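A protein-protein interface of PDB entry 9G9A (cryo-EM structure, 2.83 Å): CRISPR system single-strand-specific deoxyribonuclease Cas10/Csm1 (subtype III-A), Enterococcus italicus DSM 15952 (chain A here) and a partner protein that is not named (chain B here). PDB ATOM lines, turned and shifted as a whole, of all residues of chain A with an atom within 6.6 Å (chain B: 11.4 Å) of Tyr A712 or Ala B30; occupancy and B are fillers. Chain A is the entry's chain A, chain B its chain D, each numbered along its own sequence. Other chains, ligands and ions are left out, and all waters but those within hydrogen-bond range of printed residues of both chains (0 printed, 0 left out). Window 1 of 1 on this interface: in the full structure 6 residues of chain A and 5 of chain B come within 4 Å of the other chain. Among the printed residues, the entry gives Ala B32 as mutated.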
ATOM      1  N   GLY A 707      12.799  25.795 -23.478  1.00  0.00           N
ATOM      2  CA  GLY A 707      12.302  24.482 -23.099  1.00  0.00           C
ATOM      3  C   GLY A 707      11.897  24.365 -21.646  1.00  0.00           C
ATOM      4  O   GLY A 707      12.168  23.340 -21.009  1.00  0.00           O
ATOM      5  N   LYS A 708      11.253  25.400 -21.101  1.00  0.00           N
ATOM      6  CA  LYS A 708      10.823  25.347 -19.707  1.00  0.00           C
ATOM      7  C   LYS A 708       9.662  24.375 -19.526  1.00  0.00           C
ATOM      8  O   LYS A 708       9.624  23.612 -18.553  1.00  0.00           O
ATOM      9  CB  LYS A 708      10.442  26.746 -19.224  1.00  0.00           C
ATOM     10  CG  LYS A 708      10.120  26.822 -17.742  1.00  0.00           C
ATOM     11  CD  LYS A 708       9.945  28.260 -17.288  1.00  0.00           C
ATOM     12  CE  LYS A 708       8.853  28.961 -18.079  1.00  0.00           C
ATOM     13  NZ  LYS A 708       8.666  30.372 -17.640  1.00  0.00           N
ATOM     14  N   SER A 709       8.703  24.393 -20.455  1.00  0.00           N
ATOM     15  CA  SER A 709       7.579  23.464 -20.372  1.00  0.00           C
ATOM     16  C   SER A 709       8.042  22.025 -20.554  1.00  0.00           C
ATOM     17  O   SER A 709       7.513  21.109 -19.914  1.00  0.00           O
ATOM     18  CB  SER A 709       6.521  23.829 -21.414  1.00  0.00           C
ATOM     19  OG  SER A 709       7.069  23.816 -22.721  1.00  0.00           O
ATOM     20  N   PHE A 710       9.028  21.807 -21.426  1.00  0.00           N
ATOM     21  CA  PHE A 710       9.593  20.473 -21.595  1.00  0.00           C
ATOM     22  C   PHE A 710      10.231  19.980 -20.301  1.00  0.00           C
ATOM     23  O   PHE A 710      10.065  18.819 -19.910  1.00  0.00           O
ATOM     24  CB  PHE A 710      10.610  20.488 -22.736  1.00  0.00           C
ATOM     25  CG  PHE A 710      11.419  19.231 -22.844  1.00  0.00           C
ATOM     26  CD1 PHE A 710      10.797  18.008 -23.016  1.00  0.00           C
ATOM     27  CD2 PHE A 710      12.800  19.276 -22.788  1.00  0.00           C
ATOM     28  CE1 PHE A 710      11.538  16.852 -23.116  1.00  0.00           C
ATOM     29  CE2 PHE A 710      13.547  18.121 -22.892  1.00  0.00           C
ATOM     30  CZ  PHE A 710      12.915  16.908 -23.057  1.00  0.00           C
ATOM     31  N   LEU A 711      10.964  20.861 -19.617  1.00  0.00           N
ATOM     32  CA  LEU A 711      11.556  20.496 -18.336  1.00  0.00           C
ATOM     33  C   LEU A 711      10.496  20.236 -17.277  1.00  0.00           C
ATOM     34  O   LEU A 711      10.666  19.343 -16.441  1.00  0.00           O
ATOM     35  CB  LEU A 711      12.512  21.588 -17.868  1.00  0.00           C
ATOM     36  CG  LEU A 711      13.803  21.745 -18.666  1.00  0.00           C
ATOM     37  CD1 LEU A 711      14.610  22.907 -18.127  1.00  0.00           C
ATOM     38  CD2 LEU A 711      14.612  20.460 -18.621  1.00  0.00           C
ATOM     39  N   TYR A 712       9.404  21.002 -17.288  1.00  0.00           N
ATOM     40  CA  TYR A 712       8.316  20.741 -16.349  1.00  0.00           C
ATOM     41  C   TYR A 712       7.673  19.384 -16.612  1.00  0.00           C
ATOM     42  O   TYR A 712       7.330  18.659 -15.668  1.00  0.00           O
ATOM     43  CB  TYR A 712       7.278  21.859 -16.428  1.00  0.00           C
ATOM     44  CG  TYR A 712       7.633  23.076 -15.605  1.00  0.00           C
ATOM     45  CD1 TYR A 712       8.113  22.946 -14.310  1.00  0.00           C
ATOM     46  CD2 TYR A 712       7.491  24.355 -16.125  1.00  0.00           C
ATOM     47  CE1 TYR A 712       8.438  24.053 -13.552  1.00  0.00           C
ATOM     48  CE2 TYR A 712       7.814  25.469 -15.374  1.00  0.00           C
ATOM     49  CZ  TYR A 712       8.288  25.311 -14.090  1.00  0.00           C
ATOM     50  OH  TYR A 712       8.612  26.417 -13.339  1.00  0.00           O
ATOM     51  N   LYS A 713       7.493  19.029 -17.886  1.00  0.00           N
ATOM     52  CA  LYS A 713       6.972  17.706 -18.218  1.00  0.00           C
ATOM     53  C   LYS A 713       7.925  16.608 -17.760  1.00  0.00           C
ATOM     54  O   LYS A 713       7.491  15.584 -17.219  1.00  0.00           O
ATOM     55  CB  LYS A 713       6.714  17.604 -19.721  1.00  0.00           C
ATOM     56  CG  LYS A 713       5.596  18.506 -20.213  1.00  0.00           C
ATOM     57  CD  LYS A 713       5.464  18.462 -21.725  1.00  0.00           C
ATOM     58  CE  LYS A 713       4.338  19.364 -22.200  1.00  0.00           C
ATOM     59  NZ  LYS A 713       4.521  20.772 -21.748  1.00  0.00           N
ATOM     60  N   MET A 714       9.229  16.806 -17.963  1.00  0.00           N
ATOM     61  CA  MET A 714      10.202  15.834 -17.475  1.00  0.00           C
ATOM     62  C   MET A 714      10.125  15.696 -15.961  1.00  0.00           C
ATOM     63  O   MET A 714      10.186  14.582 -15.428  1.00  0.00           O
ATOM     64  CB  MET A 714      11.614  16.234 -17.898  1.00  0.00           C
ATOM     65  CG  MET A 714      11.876  16.155 -19.386  1.00  0.00           C
ATOM     66  SD  MET A 714      13.609  16.465 -19.768  1.00  0.00           S
ATOM     67  CE  MET A 714      14.375  15.064 -18.966  1.00  0.00           C
ATOM     68  N   LEU A 715       9.991  16.817 -15.250  1.00  0.00           N
ATOM     69  CA  LEU A 715       9.903  16.774 -13.794  1.00  0.00           C
ATOM     70  C   LEU A 715       8.659  16.025 -13.336  1.00  0.00           C
ATOM     71  O   LEU A 715       8.721  15.200 -12.419  1.00  0.00           O
ATOM     72  CB  LEU A 715       9.906  18.194 -13.229  1.00  0.00           C
ATOM     73  CG  LEU A 715      11.273  18.822 -12.964  1.00  0.00           C
ATOM     74  CD1 LEU A 715      11.123  20.290 -12.617  1.00  0.00           C
ATOM     75  CD2 LEU A 715      11.987  18.077 -11.851  1.00  0.00           C
ATOM     76  N   GLU A 716       7.514  16.299 -13.966  1.00  0.00           N
ATOM     77  CA  GLU A 716       6.283  15.641 -13.541  1.00  0.00           C
ATOM     78  C   GLU A 716       6.285  14.162 -13.907  1.00  0.00           C
ATOM     79  O   GLU A 716       5.637  13.358 -13.229  1.00  0.00           O
ATOM     80  CB  GLU A 716       5.063  16.350 -14.131  1.00  0.00           C
ATOM     81  CG  GLU A 716       4.910  16.229 -15.634  1.00  0.00           C
ATOM     82  CD  GLU A 716       3.738  15.356 -16.035  1.00  0.00           C
ATOM     83  OE1 GLU A 716       2.930  14.995 -15.154  1.00  0.00           O
ATOM     84  OE2 GLU A 716       3.623  15.031 -17.236  1.00  0.00           O
ATOM     85  N   LEU A 717       7.004  13.782 -14.967  1.00  0.00           N
ATOM     86  CA  LEU A 717       7.156  12.362 -15.272  1.00  0.00           C
ATOM     87  C   LEU A 717       8.102  11.681 -14.289  1.00  0.00           C
ATOM     88  O   LEU A 717       7.871  10.534 -13.890  1.00  0.00           O
ATOM     89  CB  LEU A 717       7.647  12.182 -16.707  1.00  0.00           C
ATOM     90  CG  LEU A 717       6.618  12.476 -17.800  1.00  0.00           C
ATOM     91  CD1 LEU A 717       7.237  12.332 -19.175  1.00  0.00           C
ATOM     92  CD2 LEU A 717       5.414  11.561 -17.656  1.00  0.00           C
ATOM     93  N   ARG A 719       8.704  12.578 -11.169  1.00  0.00           N
ATOM     94  CA  ARG A 719       8.124  12.504  -9.832  1.00  0.00           C
ATOM     95  C   ARG A 719       7.330  11.224  -9.616  1.00  0.00           C
ATOM     96  O   ARG A 719       7.088  10.846  -8.465  1.00  0.00           O
ATOM     97  CB  ARG A 719       7.224  13.712  -9.565  1.00  0.00           C
ATOM     98  CG  ARG A 719       7.962  15.029  -9.392  1.00  0.00           C
ATOM     99  CD  ARG A 719       7.011  16.130  -8.948  1.00  0.00           C
ATOM    100  NE  ARG A 719       7.609  17.453  -9.072  1.00  0.00           N
ATOM    101  CZ  ARG A 719       7.391  18.281 -10.084  1.00  0.00           C
ATOM    102  NH1 ARG A 719       6.573  17.961 -11.074  1.00  0.00           N
ATOM    103  NH2 ARG A 719       8.006  19.459 -10.104  1.00  0.00           N
ATOM    104  N   ILE A 763      17.552  19.245 -13.565  1.00  0.00           N
ATOM    105  CA  ILE A 763      16.406  19.836 -14.249  1.00  0.00           C
ATOM    106  C   ILE A 763      15.849  21.005 -13.447  1.00  0.00           C
ATOM    107  O   ILE A 763      15.514  22.054 -14.008  1.00  0.00           O
ATOM    108  CB  ILE A 763      15.328  18.770 -14.518  1.00  0.00           C
ATOM    109  CG1 ILE A 763      15.850  17.718 -15.496  1.00  0.00           C
ATOM    110  CG2 ILE A 763      14.076  19.414 -15.081  1.00  0.00           C
ATOM    111  CD1 ILE A 763      14.899  16.565 -15.706  1.00  0.00           C
ATOM    112  N   GLU A 764      15.738  20.844 -12.127  1.00  0.00           N
ATOM    113  CA  GLU A 764      15.251  21.936 -11.289  1.00  0.00           C
ATOM    114  C   GLU A 764      16.200  23.126 -11.328  1.00  0.00           C
ATOM    115  O   GLU A 764      15.757  24.280 -11.372  1.00  0.00           O
ATOM    116  CB  GLU A 764      15.056  21.456  -9.851  1.00  0.00           C
ATOM    117  CG  GLU A 764      13.952  20.431  -9.682  1.00  0.00           C
ATOM    118  CD  GLU A 764      13.678  20.112  -8.229  1.00  0.00           C
ATOM    119  OE1 GLU A 764      13.943  20.979  -7.371  1.00  0.00           O
ATOM    120  OE2 GLU A 764      13.201  18.993  -7.942  1.00  0.00           O
ATOM    121  N   VAL A 767      15.658  24.862 -14.613  1.00  0.00           N
ATOM    122  CA  VAL A 767      14.387  25.580 -14.586  1.00  0.00           C
ATOM    123  C   VAL A 767      14.535  26.885 -13.819  1.00  0.00           C
ATOM    124  O   VAL A 767      14.116  27.951 -14.285  1.00  0.00           O
ATOM    125  CB  VAL A 767      13.282  24.696 -13.979  1.00  0.00           C
ATOM    126  CG1 VAL A 767      12.076  25.538 -13.605  1.00  0.00           C
ATOM    127  CG2 VAL A 767      12.876  23.611 -14.953  1.00  0.00           C
ATOM    128  N   TYR A 768      15.155  26.823 -12.638  1.00  0.00           N
ATOM    129  CA  TYR A 768      15.376  28.032 -11.854  1.00  0.00           C
ATOM    130  C   TYR A 768      16.275  29.019 -12.585  1.00  0.00           C
ATOM    131  O   TYR A 768      16.137  30.232 -12.404  1.00  0.00           O
ATOM    132  CB  TYR A 768      15.981  27.673 -10.498  1.00  0.00           C
ATOM    133  CG  TYR A 768      15.060  26.889  -9.593  1.00  0.00           C
ATOM    134  CD1 TYR A 768      13.695  27.128  -9.582  1.00  0.00           C
ATOM    135  CD2 TYR A 768      15.560  25.909  -8.750  1.00  0.00           C
ATOM    136  CE1 TYR A 768      12.853  26.413  -8.755  1.00  0.00           C
ATOM    137  CE2 TYR A 768      14.726  25.188  -7.922  1.00  0.00           C
ATOM    138  CZ  TYR A 768      13.375  25.443  -7.927  1.00  0.00           C
ATOM    139  OH  TYR A 768      12.544  24.725  -7.101  1.00  0.00           O
ATOM    140  N   ARG A 771      14.027  30.782 -15.433  1.00  0.00           N
ATOM    141  CA  ARG A 771      12.820  31.487 -15.033  1.00  0.00           C
ATOM    142  C   ARG A 771      12.923  32.971 -15.377  1.00  0.00           C
ATOM    143  O   ARG A 771      14.009  33.515 -15.596  1.00  0.00           O
ATOM    144  CB  ARG A 771      12.567  31.321 -13.534  1.00  0.00           C
ATOM    145  CG  ARG A 771      12.099  29.939 -13.128  1.00  0.00           C
ATOM    146  CD  ARG A 771      10.619  29.747 -13.396  1.00  0.00           C
ATOM    147  NE  ARG A 771       9.803  30.261 -12.303  1.00  0.00           N
ATOM    148  CZ  ARG A 771       9.484  29.567 -11.219  1.00  0.00           C
ATOM    149  NH1 ARG A 771       9.905  28.325 -11.046  1.00  0.00           N
ATOM    150  NH2 ARG A 771       8.722  30.132 -10.288  1.00  0.00           N
ATOM    151  N   GLY B  29       8.525  19.278  -6.106  1.00  0.00           N
ATOM    152  CA  GLY B  29       9.545  19.759  -7.019  1.00  0.00           C
ATOM    153  C   GLY B  29       9.260  21.147  -7.555  1.00  0.00           C
ATOM    154  O   GLY B  29       8.521  21.919  -6.943  1.00  0.00           O
ATOM    155  N   ALA B  30       9.849  21.468  -8.704  1.00  0.00           N
ATOM    156  CA  ALA B  30       9.653  22.769  -9.332  1.00  0.00           C
ATOM    157  C   ALA B  30       8.358  22.737 -10.136  1.00  0.00           C
ATOM    158  O   ALA B  30       8.248  22.003 -11.122  1.00  0.00           O
ATOM    159  CB  ALA B  30      10.843  23.124 -10.216  1.00  0.00           C
ATOM    160  N   ILE B  31       7.377  23.530  -9.712  1.00  0.00           N
ATOM    161  CA  ILE B  31       6.075  23.602 -10.362  1.00  0.00           C
ATOM    162  C   ILE B  31       5.733  25.066 -10.594  1.00  0.00           C
ATOM    163  O   ILE B  31       5.932  25.906  -9.709  1.00  0.00           O
ATOM    164  CB  ILE B  31       4.978  22.911  -9.523  1.00  0.00           C
ATOM    165  CG1 ILE B  31       5.279  21.421  -9.367  1.00  0.00           C
ATOM    166  CG2 ILE B  31       3.612  23.108 -10.155  1.00  0.00           C
ATOM    167  CD1 ILE B  31       4.235  20.669  -8.576  1.00  0.00           C
ATOM    168  N   ALA B  32       5.227  25.372 -11.786  1.00  0.00           N
ATOM    169  CA  ALA B  32       4.789  26.724 -12.105  1.00  0.00           C
ATOM    170  C   ALA B  32       3.392  26.950 -11.541  1.00  0.00           C
ATOM    171  O   ALA B  32       2.451  26.228 -11.890  1.00  0.00           O
ATOM    172  CB  ALA B  32       4.807  26.949 -13.616  1.00  0.00           C
ATOM    173  N   SER B  33       3.261  27.952 -10.670  1.00  0.00           N
ATOM    174  CA  SER B  33       2.021  28.298  -9.983  1.00  0.00           C
ATOM    175  C   SER B  33       1.447  27.100  -9.233  1.00  0.00           C
ATOM    176  O   SER B  33       0.369  26.608  -9.589  1.00  0.00           O
ATOM    177  CB  SER B  33       0.992  28.842 -10.977  1.00  0.00           C
ATOM    178  OG  SER B  33       1.493  29.971 -11.669  1.00  0.00           O
ATOM    179  N   PRO B  34       2.123  26.605  -8.199  1.00  0.00           N
ATOM    180  CA  PRO B  34       1.595  25.458  -7.456  1.00  0.00           C
ATOM    181  C   PRO B  34       0.411  25.840  -6.582  1.00  0.00           C
ATOM    182  O   PRO B  34       0.241  26.994  -6.184  1.00  0.00           O
ATOM    183  CB  PRO B  34       2.785  25.014  -6.591  1.00  0.00           C
ATOM    184  CG  PRO B  34       3.971  25.786  -7.099  1.00  0.00           C
ATOM    185  CD  PRO B  34       3.419  27.044  -7.662  1.00  0.00           C
ATOM    186  N   VAL B  35      -0.413  24.839  -6.284  1.00  0.00           N
ATOM    187  CA  VAL B  35      -1.494  25.024  -5.326  1.00  0.00           C
ATOM    188  C   VAL B  35      -0.974  24.782  -3.914  1.00  0.00           C
ATOM    189  O   VAL B  35       0.086  24.188  -3.702  1.00  0.00           O
ATOM    190  CB  VAL B  35      -2.687  24.105  -5.643  1.00  0.00           C
ATOM    191  CG1 VAL B  35      -3.345  24.519  -6.941  1.00  0.00           C
ATOM    192  CG2 VAL B  35      -2.240  22.655  -5.705  1.00  0.00           C
ATOM    193  N   ARG B  37      -0.663  22.918  -0.567  1.00  0.00           N
ATOM    194  CA  ARG B  37      -0.725  21.496  -0.274  1.00  0.00           C
ATOM    195  C   ARG B  37      -0.366  21.251   1.182  1.00  0.00           C
ATOM    196  O   ARG B  37       0.338  22.048   1.808  1.00  0.00           O
ATOM    197  CB  ARG B  37       0.220  20.697  -1.179  1.00  0.00           C
ATOM    198  CG  ARG B  37      -0.423  20.169  -2.445  1.00  0.00           C
ATOM    199  CD  ARG B  37       0.579  19.399  -3.281  1.00  0.00           C
ATOM    200  NE  ARG B  37       1.400  20.284  -4.098  1.00  0.00           N
ATOM    201  CZ  ARG B  37       1.239  20.454  -5.402  1.00  0.00           C
ATOM    202  NH1 ARG B  37       0.313  19.792  -6.075  1.00  0.00           N
ATOM    203  NH2 ARG B  37       2.031  21.305  -6.049  1.00  0.00           N
ATOM    204  N   ARG B  42       1.235  15.952   1.177  1.00  0.00           N
ATOM    205  CA  ARG B  42       1.336  16.537  -0.162  1.00  0.00           C
ATOM    206  C   ARG B  42      -0.011  16.521  -0.882  1.00  0.00           C
ATOM    207  O   ARG B  42      -0.078  16.460  -2.110  1.00  0.00           O
ATOM    208  CB  ARG B  42       2.409  15.835  -0.999  1.00  0.00           C
ATOM    209  CG  ARG B  42       3.842  16.161  -0.605  1.00  0.00           C
ATOM    210  CD  ARG B  42       4.237  17.574  -1.020  1.00  0.00           C
ATOM    211  NE  ARG B  42       3.899  18.571  -0.010  1.00  0.00           N
ATOM    212  CZ  ARG B  42       4.068  19.878  -0.161  1.00  0.00           C
ATOM    213  NH1 ARG B  42       4.558  20.387  -1.279  1.00  0.00           N
ATOM    214  NH2 ARG B  42       3.738  20.694   0.834  1.00  0.00           N
ATOM    215  N   THR B 119      -4.152  16.729  -9.118  1.00  0.00           N
ATOM    216  CA  THR B 119      -4.018  18.067  -9.670  1.00  0.00           C
ATOM    217  C   THR B 119      -3.741  17.987 -11.164  1.00  0.00           C
ATOM    218  O   THR B 119      -3.203  17.000 -11.672  1.00  0.00           O
ATOM    219  CB  THR B 119      -2.900  18.863  -8.979  1.00  0.00           C
ATOM    220  OG1 THR B 119      -1.681  18.110  -9.009  1.00  0.00           O
ATOM    221  CG2 THR B 119      -3.271  19.171  -7.538  1.00  0.00           C
ATOM    222  N   GLU B 120      -4.121  19.054 -11.859  1.00  0.00           N
ATOM    223  CA  GLU B 120      -3.923  19.194 -13.292  1.00  0.00           C
ATOM    224  C   GLU B 120      -3.145  20.472 -13.566  1.00  0.00           C
ATOM    225  O   GLU B 120      -3.101  21.387 -12.741  1.00  0.00           O
ATOM    226  CB  GLU B 120      -5.258  19.231 -14.047  1.00  0.00           C
ATOM    227  CG  GLU B 120      -6.217  20.288 -13.525  1.00  0.00           C
ATOM    228  CD  GLU B 120      -7.212  20.745 -14.571  1.00  0.00           C
ATOM    229  OE1 GLU B 120      -6.858  20.750 -15.768  1.00  0.00           O
ATOM    230  OE2 GLU B 120      -8.350  21.097 -14.197  1.00  0.00           O
ATOM    231  N   THR B 121      -2.527  20.527 -14.740  1.00  0.00           N
ATOM    232  CA  THR B 121      -1.789  21.706 -15.185  1.00  0.00           C
ATOM    233  C   THR B 121      -2.605  22.380 -16.282  1.00  0.00           C
ATOM    234  O   THR B 121      -2.662  21.897 -17.415  1.00  0.00           O
ATOM    235  CB  THR B 121      -0.397  21.329 -15.677  1.00  0.00           C
ATOM    236  OG1 THR B 121       0.338  20.717 -14.611  1.00  0.00           O
ATOM    237  CG2 THR B 121       0.352  22.561 -16.156  1.00  0.00           C
ATOM    238  N   LYS B 122      -3.247  23.495 -15.940  1.00  0.00           N
ATOM    239  CA  LYS B 122      -3.997  24.273 -16.911  1.00  0.00           C
ATOM    240  C   LYS B 122      -3.044  25.191 -17.663  1.00  0.00           C
ATOM    241  O   LYS B 122      -2.288  25.956 -17.050  1.00  0.00           O
ATOM    242  CB  LYS B 122      -5.089  25.085 -16.216  1.00  0.00           C
ATOM    243  CG  LYS B 122      -6.040  25.798 -17.163  1.00  0.00           C
ATOM    244  CD  LYS B 122      -7.139  26.513 -16.400  1.00  0.00           C
ATOM    245  CE  LYS B 122      -8.204  27.060 -17.337  1.00  0.00           C
ATOM    246  NZ  LYS B 122      -7.672  28.108 -18.248  1.00  0.00           N
ATOM    247  N   PHE B 123      -3.076  25.101 -18.988  1.00  0.00           N
ATOM    248  CA  PHE B 123      -2.213  25.884 -19.861  1.00  0.00           C
ATOM    249  C   PHE B 123      -3.009  27.047 -20.434  1.00  0.00           C
ATOM    250  O   PHE B 123      -4.086  26.850 -21.007  1.00  0.00           O
ATOM    251  CB  PHE B 123      -1.653  25.021 -20.992  1.00  0.00           C
ATOM    252  CG  PHE B 123      -0.722  23.935 -20.531  1.00  0.00           C
ATOM    253  CD1 PHE B 123      -1.216  22.718 -20.094  1.00  0.00           C
ATOM    254  CD2 PHE B 123       0.647  24.125 -20.553  1.00  0.00           C
ATOM    255  CE1 PHE B 123      -0.361  21.717 -19.675  1.00  0.00           C
ATOM    256  CE2 PHE B 123       1.506  23.129 -20.136  1.00  0.00           C
ATOM    257  CZ  PHE B 123       1.001  21.923 -19.696  1.00  0.00           C
ATOM    258  N   PRO B 136       2.813  32.195 -23.013  1.00  0.00           N
ATOM    259  CA  PRO B 136       2.383  30.961 -22.346  1.00  0.00           C
ATOM    260  C   PRO B 136       2.478  31.064 -20.831  1.00  0.00           C
ATOM    261  O   PRO B 136       3.343  31.753 -20.283  1.00  0.00           O
ATOM    262  CB  PRO B 136       3.348  29.906 -22.896  1.00  0.00           C
ATOM    263  CG  PRO B 136       4.537  30.680 -23.352  1.00  0.00           C
ATOM    264  CD  PRO B 136       4.005  31.985 -23.851  1.00  0.00           C
ATOM    265  N   ARG B 137       1.567  30.364 -20.160  1.00  0.00           N
ATOM    266  CA  ARG B 137       1.463  30.357 -18.710  1.00  0.00           C
ATOM    267  C   ARG B 137       0.883  29.019 -18.279  1.00  0.00           C
ATOM    268  O   ARG B 137       0.102  28.411 -19.014  1.00  0.00           O
ATOM    269  CB  ARG B 137       0.580  31.515 -18.220  1.00  0.00           C
ATOM    270  CG  ARG B 137       0.446  31.633 -16.715  1.00  0.00           C
ATOM    271  CD  ARG B 137      -0.367  32.857 -16.321  1.00  0.00           C
ATOM    272  NE  ARG B 137      -1.763  32.766 -16.733  1.00  0.00           N
ATOM    273  CZ  ARG B 137      -2.269  33.355 -17.809  1.00  0.00           C
ATOM    274  NH1 ARG B 137      -1.515  34.077 -18.621  1.00  0.00           N
ATOM    275  NH2 ARG B 137      -3.564  33.216 -18.075  1.00  0.00           N
ATOM    276  N   GLN B 138       1.270  28.554 -17.094  1.00  0.00           N
ATOM    277  CA  GLN B 138       0.773  27.301 -16.543  1.00  0.00           C
ATOM    278  C   GLN B 138       0.356  27.525 -15.099  1.00  0.00           C
ATOM    279  O   GLN B 138       1.063  28.202 -14.346  1.00  0.00           O
ATOM    280  CB  GLN B 138       1.835  26.201 -16.617  1.00  0.00           C
ATOM    281  CG  GLN B 138       2.393  25.960 -18.005  1.00  0.00           C
ATOM    282  CD  GLN B 138       3.468  24.896 -18.016  1.00  0.00           C
ATOM    283  OE1 GLN B 138       3.647  24.169 -17.039  1.00  0.00           O
ATOM    284  NE2 GLN B 138       4.195  24.802 -19.123  1.00  0.00           N
ATOM    285  N   ILE B 139      -0.788  26.964 -14.714  1.00  0.00           N
ATOM    286  CA  ILE B 139      -1.272  27.047 -13.341  1.00  0.00           C
ATOM    287  C   ILE B 139      -1.709  25.661 -12.890  1.00  0.00           C
ATOM    288  O   ILE B 139      -2.399  24.950 -13.628  1.00  0.00           O
ATOM    289  CB  ILE B 139      -2.425  28.058 -13.192  1.00  0.00           C
ATOM    290  CG1 ILE B 139      -3.541  27.766 -14.196  1.00  0.00           C
ATOM    291  CG2 ILE B 139      -1.915  29.480 -13.358  1.00  0.00           C
ATOM    292  CD1 ILE B 139      -4.805  28.549 -13.942  1.00  0.00           C
ATOM    293  N   GLU B 140      -1.299  25.272 -11.689  1.00  0.00           N
ATOM    294  CA  GLU B 140      -1.807  24.040 -11.107  1.00  0.00           C
ATOM    295  C   GLU B 140      -3.216  24.263 -10.574  1.00  0.00           C
ATOM    296  O   GLU B 140      -3.521  25.315 -10.006  1.00  0.00           O
ATOM    297  CB  GLU B 140      -0.884  23.557  -9.992  1.00  0.00           C
ATOM    298  CG  GLU B 140      -1.169  22.146  -9.522  1.00  0.00           C
ATOM    299  CD  GLU B 140      -0.065  21.592  -8.650  1.00  0.00           C
ATOM    300  OE1 GLU B 140       0.890  22.339  -8.355  1.00  0.00           O
ATOM    301  OE2 GLU B 140      -0.147  20.409  -8.262  1.00  0.00           O
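Printed residues of chain B within 4 Å of Tyr A712: Ala B30, Ile B31, Ala B32 and Gln B138. Ala B30 touches four residues of chain A. No residue of chain B comes within 4 Å of Lys A708. No residue of chain B comes within 4 Å of Leu A711. No residue of chain B comes within 4 Å of Lys A713. Leu A715 touches one residue of chain B. Of chain B, only Gly B29 (3.8 Å) comes within 4 Å of Glu A764. Val A767 touches none of the printed residues of chain B. Of the printed residues of chain B, Arg A719 touches Gly B29 (3.3 Å), Ala B30 (2.8 Å) and Ile B31 (3.4 Å). Printed residues of chain B within 4 Å of Tyr A768: Ala B30 (3.9 Å). Of the printed residues of chain A, Gln B138 touches Ser A709 (3.4 Å) and Tyr A712 (3.96 Å). Printed residues of chain A within 4 Å of Gly B29: Arg A719 and Glu A764. Of the printed residues of chain A, Ile B31 touches Tyr A712 and Arg A719. The nearest printed residue of chain B that does not touch Tyr A712 is Ser B33 (6.2 Å). The nearest residue of chain A that does not touch Ala B30 is Glu A764 (4.1 Å). The nearest printed residue of chain A that does not touch Ala B32 is Arg A771 (5.5 Å).
The guanidinium group of Arg A719 is in hydrogen-bond range of the backbone carbonyl oxygen of Ala B30 (2.8 Å).
CB of Ser A709 touches NE2 of Gln B138, at 3.4 Å. CE1 of Tyr A712 touches O of Ala B30, at 3.2 Å. CA of Ile B31 touches CE1 of Tyr A712 (3.995 Å). CB of Ala B32 touches CE2 of Tyr A712, at 3.8 Å. Tyr A712 touches Gln B138. O of Ala B30 touches CD1 of Leu A715 (3.7 Å). Gly B29 touches Arg A719. Arg A719 touches Ile B31 (NH2 to CG1, 3.4 Å). Glu A764 touches Gly B29. Tyr A768 touches Ala B30.
Of the 17 printed residues of chain A, 6 touch a printed residue of chain B. Hydrophobic or aromatic side chains of chain B within 4 Å of the printed part of chain A: Ala B30, Ile B31 and Ala B32. Among the printed residues, 11 pairs touch across the chains. Among the printed residues, no Asp or Glu carboxylate lies within 4 Å of a Lys or Arg side-chain nitrogen of the other chain.
The side-chain hydroxyl (OH) of Tyr A712 lies within hydrogen-bond range of the guanidinium group (NH1) of Arg A771, at 3.3 Å. O of Gln B138 sits at hydrogen-bond distance from OG of Ser B33 (3.2 Å).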
